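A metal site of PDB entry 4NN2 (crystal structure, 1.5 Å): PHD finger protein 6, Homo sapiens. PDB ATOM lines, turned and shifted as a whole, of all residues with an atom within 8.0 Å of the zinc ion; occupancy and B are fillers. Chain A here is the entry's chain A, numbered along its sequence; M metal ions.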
ATOM      1  N   GLY A  87      28.067 -11.870  -2.286  1.00  0.00           N
ATOM      2  CA  GLY A  87      28.946 -10.715  -2.205  1.00  0.00           C
ATOM      3  C   GLY A  87      28.969  -9.920  -3.492  1.00  0.00           C
ATOM      4  O   GLY A  87      28.833 -10.480  -4.571  1.00  0.00           O
ATOM      5  N   CYS A  88      29.151  -8.612  -3.382  1.00  0.00           N
ATOM      6  CA  CYS A  88      29.345  -7.791  -4.559  1.00  0.00           C
ATOM      7  C   CYS A  88      30.542  -8.327  -5.331  1.00  0.00           C
ATOM      8  O   CYS A  88      31.551  -8.706  -4.753  1.00  0.00           O
ATOM      9  CB  CYS A  88      29.581  -6.337  -4.158  1.00  0.00           C
ATOM     10  SG  CYS A  88      29.761  -5.222  -5.576  1.00  0.00           S
ATOM     11  N   GLU A  89      30.393  -8.373  -6.644  1.00  0.00           N
ATOM     12  CA  GLU A  89      31.413  -8.940  -7.524  1.00  0.00           C
ATOM     13  C   GLU A  89      32.723  -8.145  -7.501  1.00  0.00           C
ATOM     14  O   GLU A  89      33.796  -8.688  -7.773  1.00  0.00           O
ATOM     15  CB  GLU A  89      30.873  -8.995  -8.949  1.00  0.00           C
ATOM     16  CG  GLU A  89      31.704  -9.816  -9.909  1.00  0.00           C
ATOM     17  CD  GLU A  89      31.586 -11.321  -9.706  1.00  0.00           C
ATOM     18  OE1 GLU A  89      30.827 -11.791  -8.812  1.00  0.00           O
ATOM     19  OE2 GLU A  89      32.249 -12.035 -10.479  1.00  0.00           O
ATOM     20  N   ILE A  90      32.650  -6.845  -7.205  1.00  0.00           N
ATOM     21  CA  ILE A  90      33.853  -6.006  -7.176  1.00  0.00           C
ATOM     22  C   ILE A  90      34.733  -6.478  -6.003  1.00  0.00           C
ATOM     23  O   ILE A  90      34.290  -6.521  -4.859  1.00  0.00           O
ATOM     24  CB  ILE A  90      33.480  -4.511  -7.073  1.00  0.00           C
ATOM     25  CG1 ILE A  90      32.664  -4.051  -8.299  1.00  0.00           C
ATOM     26  CG2 ILE A  90      34.725  -3.653  -6.908  1.00  0.00           C
ATOM     27  CD1 ILE A  90      33.275  -4.368  -9.663  1.00  0.00           C
ATOM     28  N   LYS A  91      35.978  -6.850  -6.286  1.00  0.00           N
ATOM     29  CA  LYS A  91      36.748  -7.691  -5.329  1.00  0.00           C
ATOM     30  C   LYS A  91      36.861  -7.167  -3.866  1.00  0.00           C
ATOM     31  O   LYS A  91      36.635  -7.942  -2.909  1.00  0.00           O
ATOM     32  CB  LYS A  91      38.130  -8.019  -5.893  1.00  0.00           C
ATOM     33  CG  LYS A  91      38.074  -9.019  -7.043  1.00  0.00           C
ATOM     34  CD  LYS A  91      39.455  -9.293  -7.609  1.00  0.00           C
ATOM     35  CE  LYS A  91      39.393 -10.247  -8.788  1.00  0.00           C
ATOM     36  NZ  LYS A  91      40.708 -10.444  -9.441  1.00  0.00           N
ATOM     37  N   ALA A  92      37.196  -5.892  -3.698  1.00  0.00           N
ATOM     38  CA  ALA A  92      37.362  -5.285  -2.369  1.00  0.00           C
ATOM     39  C   ALA A  92      36.073  -4.753  -1.730  1.00  0.00           C
ATOM     40  O   ALA A  92      36.106  -4.174  -0.645  1.00  0.00           O
ATOM     41  CB  ALA A  92      38.404  -4.173  -2.442  1.00  0.00           C
ATOM     42  N   CYS A  93      34.940  -4.906  -2.402  1.00  0.00           N
ATOM     43  CA  CYS A  93      33.705  -4.349  -1.870  1.00  0.00           C
ATOM     44  C   CYS A  93      33.214  -5.249  -0.733  1.00  0.00           C
ATOM     45  O   CYS A  93      33.168  -6.466  -0.891  1.00  0.00           O
ATOM     46  CB  CYS A  93      32.642  -4.263  -2.963  1.00  0.00           C
ATOM     47  SG  CYS A  93      31.110  -3.530  -2.371  1.00  0.00           S
ATOM     48  N   VAL A  94      32.840  -4.632   0.378  1.00  0.00           N
ATOM     49  CA  VAL A  94      32.428  -5.378   1.565  1.00  0.00           C
ATOM     50  C   VAL A  94      30.942  -5.773   1.562  1.00  0.00           C
ATOM     51  O   VAL A  94      30.507  -6.526   2.432  1.00  0.00           O
ATOM     52  CB  VAL A  94      32.742  -4.638   2.884  1.00  0.00           C
ATOM     53  CG1 VAL A  94      34.229  -4.325   2.995  1.00  0.00           C
ATOM     54  CG2 VAL A  94      31.908  -3.388   3.047  1.00  0.00           C
ATOM     55  N   LYS A  95      30.161  -5.245   0.632  1.00  0.00           N
ATOM     56  CA  LYS A  95      28.722  -5.492   0.687  1.00  0.00           C
ATOM     57  C   LYS A  95      28.402  -6.937   0.352  1.00  0.00           C
ATOM     58  O   LYS A  95      28.950  -7.497  -0.585  1.00  0.00           O
ATOM     59  CB  LYS A  95      27.957  -4.512  -0.171  1.00  0.00           C
ATOM     60  CG  LYS A  95      28.110  -3.080   0.335  1.00  0.00           C
ATOM     61  CD  LYS A  95      26.992  -2.159  -0.129  1.00  0.00           C
ATOM     62  CE  LYS A  95      27.201  -0.733   0.346  1.00  0.00           C
ATOM     63  NZ  LYS A  95      26.649  -0.551   1.711  1.00  0.00           N
ATOM     64  N   THR A  96      27.534  -7.527   1.153  1.00  0.00           N
ATOM     65  CA  THR A  96      27.206  -8.950   0.993  1.00  0.00           C
ATOM     66  C   THR A  96      25.810  -9.191   1.536  1.00  0.00           C
ATOM     67  O   THR A  96      25.410  -8.588   2.528  1.00  0.00           O
ATOM     68  CB  THR A  96      28.277  -9.827   1.671  1.00  0.00           C
ATOM     69  OG1 THR A  96      28.124 -11.196   1.273  1.00  0.00           O
ATOM     70  CG2 THR A  96      28.272  -9.693   3.204  1.00  0.00           C
ATOM     71  N   TYR A  97      25.055 -10.063   0.868  1.00  0.00           N
ATOM     72  CA  TYR A  97      23.596 -10.094   1.062  1.00  0.00           C
ATOM     73  C   TYR A  97      22.976 -11.489   1.092  1.00  0.00           C
ATOM     74  O   TYR A  97      23.511 -12.429   0.497  1.00  0.00           O
ATOM     75  CB  TYR A  97      22.925  -9.363  -0.097  1.00  0.00           C
ATOM     76  CG  TYR A  97      23.178  -7.860  -0.136  1.00  0.00           C
ATOM     77  CD1 TYR A  97      22.453  -6.992   0.661  1.00  0.00           C
ATOM     78  CD2 TYR A  97      24.097  -7.334  -1.017  1.00  0.00           C
ATOM     79  CE1 TYR A  97      22.664  -5.607   0.599  1.00  0.00           C
ATOM     80  CE2 TYR A  97      24.312  -5.969  -1.104  1.00  0.00           C
ATOM     81  CZ  TYR A  97      23.598  -5.108  -0.293  1.00  0.00           C
ATOM     82  OH  TYR A  97      23.819  -3.741  -0.396  1.00  0.00           O
ATOM     83  N   LEU A 120      26.107 -10.412  -8.410  1.00  0.00           N
ATOM     84  CA  LEU A 120      25.483  -9.243  -7.818  1.00  0.00           C
ATOM     85  C   LEU A 120      26.469  -8.092  -7.832  1.00  0.00           C
ATOM     86  O   LEU A 120      27.644  -8.274  -7.514  1.00  0.00           O
ATOM     87  CB  LEU A 120      25.021  -9.541  -6.379  1.00  0.00           C
ATOM     88  CG  LEU A 120      24.464  -8.380  -5.548  1.00  0.00           C
ATOM     89  CD1 LEU A 120      23.478  -8.856  -4.489  1.00  0.00           C
ATOM     90  CD2 LEU A 120      25.552  -7.576  -4.854  1.00  0.00           C
ATOM     91  N   TYR A 121      25.968  -6.908  -8.171  1.00  0.00           N
ATOM     92  CA  TYR A 121      26.701  -5.670  -7.984  1.00  0.00           C
ATOM     93  C   TYR A 121      25.887  -4.818  -7.022  1.00  0.00           C
ATOM     94  O   TYR A 121      24.685  -4.619  -7.220  1.00  0.00           O
ATOM     95  CB  TYR A 121      26.877  -4.935  -9.319  1.00  0.00           C
ATOM     96  CG  TYR A 121      27.836  -5.614 -10.257  1.00  0.00           C
ATOM     97  CD1 TYR A 121      29.207  -5.501 -10.084  1.00  0.00           C
ATOM     98  CD2 TYR A 121      27.378  -6.416 -11.311  1.00  0.00           C
ATOM     99  CE1 TYR A 121      30.099  -6.128 -10.935  1.00  0.00           C
ATOM    100  CE2 TYR A 121      28.264  -7.040 -12.171  1.00  0.00           C
ATOM    101  CZ  TYR A 121      29.623  -6.913 -11.969  1.00  0.00           C
ATOM    102  OH  TYR A 121      30.510  -7.537 -12.829  1.00  0.00           O
ATOM    103  N   CYS A 122      26.524  -4.321  -5.973  1.00  0.00           N
ATOM    104  CA  CYS A 122      25.836  -3.471  -5.027  1.00  0.00           C
ATOM    105  C   CYS A 122      25.507  -2.093  -5.618  1.00  0.00           C
ATOM    106  O   CYS A 122      25.936  -1.719  -6.721  1.00  0.00           O
ATOM    107  CB  CYS A 122      26.655  -3.310  -3.748  1.00  0.00           C
ATOM    108  SG  CYS A 122      27.987  -2.080  -3.889  1.00  0.00           S
ATOM    109  N   LYS A 123      24.739  -1.326  -4.849  1.00  0.00           N
ATOM    110  CA  LYS A 123      24.294  -0.006  -5.287  1.00  0.00           C
ATOM    111  C   LYS A 123      25.428   0.967  -5.597  1.00  0.00           C
ATOM    112  O   LYS A 123      25.243   1.879  -6.399  1.00  0.00           O
ATOM    113  CB  LYS A 123      23.340   0.593  -4.257  1.00  0.00           C
ATOM    114  CG  LYS A 123      23.948   0.848  -2.885  1.00  0.00           C
ATOM    115  CD  LYS A 123      22.855   1.179  -1.872  1.00  0.00           C
ATOM    116  CE  LYS A 123      23.317   1.055  -0.443  1.00  0.00           C
ATOM    117  NZ  LYS A 123      22.178   1.302   0.499  1.00  0.00           N
ATOM    118  N   ASN A 124      26.590   0.799  -4.972  1.00  0.00           N
ATOM    119  CA  ASN A 124      27.759   1.649  -5.256  1.00  0.00           C
ATOM    120  C   ASN A 124      28.504   1.254  -6.530  1.00  0.00           C
ATOM    121  O   ASN A 124      29.311   2.032  -7.056  1.00  0.00           O
ATOM    122  CB  ASN A 124      28.748   1.598  -4.093  1.00  0.00           C
ATOM    123  CG  ASN A 124      28.177   2.168  -2.817  1.00  0.00           C
ATOM    124  OD1 ASN A 124      27.418   3.137  -2.837  1.00  0.00           O
ATOM    125  ND2 ASN A 124      28.553   1.582  -1.679  1.00  0.00           N
ATOM    126  N   HIS A 125      28.258   0.028  -6.994  1.00  0.00           N
ATOM    127  CA  HIS A 125      28.972  -0.551  -8.128  1.00  0.00           C
ATOM    128  C   HIS A 125      28.009  -0.928  -9.252  1.00  0.00           C
ATOM    129  O   HIS A 125      28.311  -1.772 -10.082  1.00  0.00           O
ATOM    130  CB  HIS A 125      29.794  -1.759  -7.653  1.00  0.00           C
ATOM    131  CG  HIS A 125      30.930  -1.375  -6.760  1.00  0.00           C
ATOM    132  ND1 HIS A 125      31.099  -1.835  -5.464  1.00  0.00           N
ATOM    133  CD2 HIS A 125      31.954  -0.519  -6.975  1.00  0.00           C
ATOM    134  CE1 HIS A 125      32.172  -1.290  -4.942  1.00  0.00           C
ATOM    135  NE2 HIS A 125      32.716  -0.492  -5.846  1.00  0.00           N
ATOM    136  N   SER A 126      26.847  -0.268  -9.271  1.00  0.00           N
ATOM    137  CA  SER A 126      25.789  -0.607 -10.215  1.00  0.00           C
ATOM    138  C   SER A 126      26.032  -0.008 -11.595  1.00  0.00           C
ATOM    139  O   SER A 126      25.454  -0.468 -12.592  1.00  0.00           O
ATOM    140  CB  SER A 126      24.432  -0.163  -9.670  1.00  0.00           C
ATOM    141  OG  SER A 126      24.431   1.213  -9.381  1.00  0.00           O
HETATM  142 ZN    ZN M   1      29.949  -3.236  -4.369  1.00  0.00          ZN
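The zinc ion is bound by ND1 of His 125 (2.1 Å), SG of Cys 122 (2.3 Å), SG of Cys 93 (2.3 Å) and SG of Cys 88 (2.3 Å).
The zinc ion has four donor atoms within binding distance.
The nearest printed residue that does not touch the zinc ion is Ile 90 (4.6 Å).
N of Lys 95 lies close to SG of Cys 93, at 3.6 Å.
The side-chain sulfur (SG) of Cys 88 sits close to the backbone NH (N) of Ile 90, at 3.7 Å.
The side-chain sulfur (SG) of Cys 122 lies close to the backbone NH (N) of Asn 124 (3.4 Å).
The backbone carbonyl oxygen of Lys 95 is in hydrogen-bond range of the backbone NH of Cys 88, at 3.0 Å.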
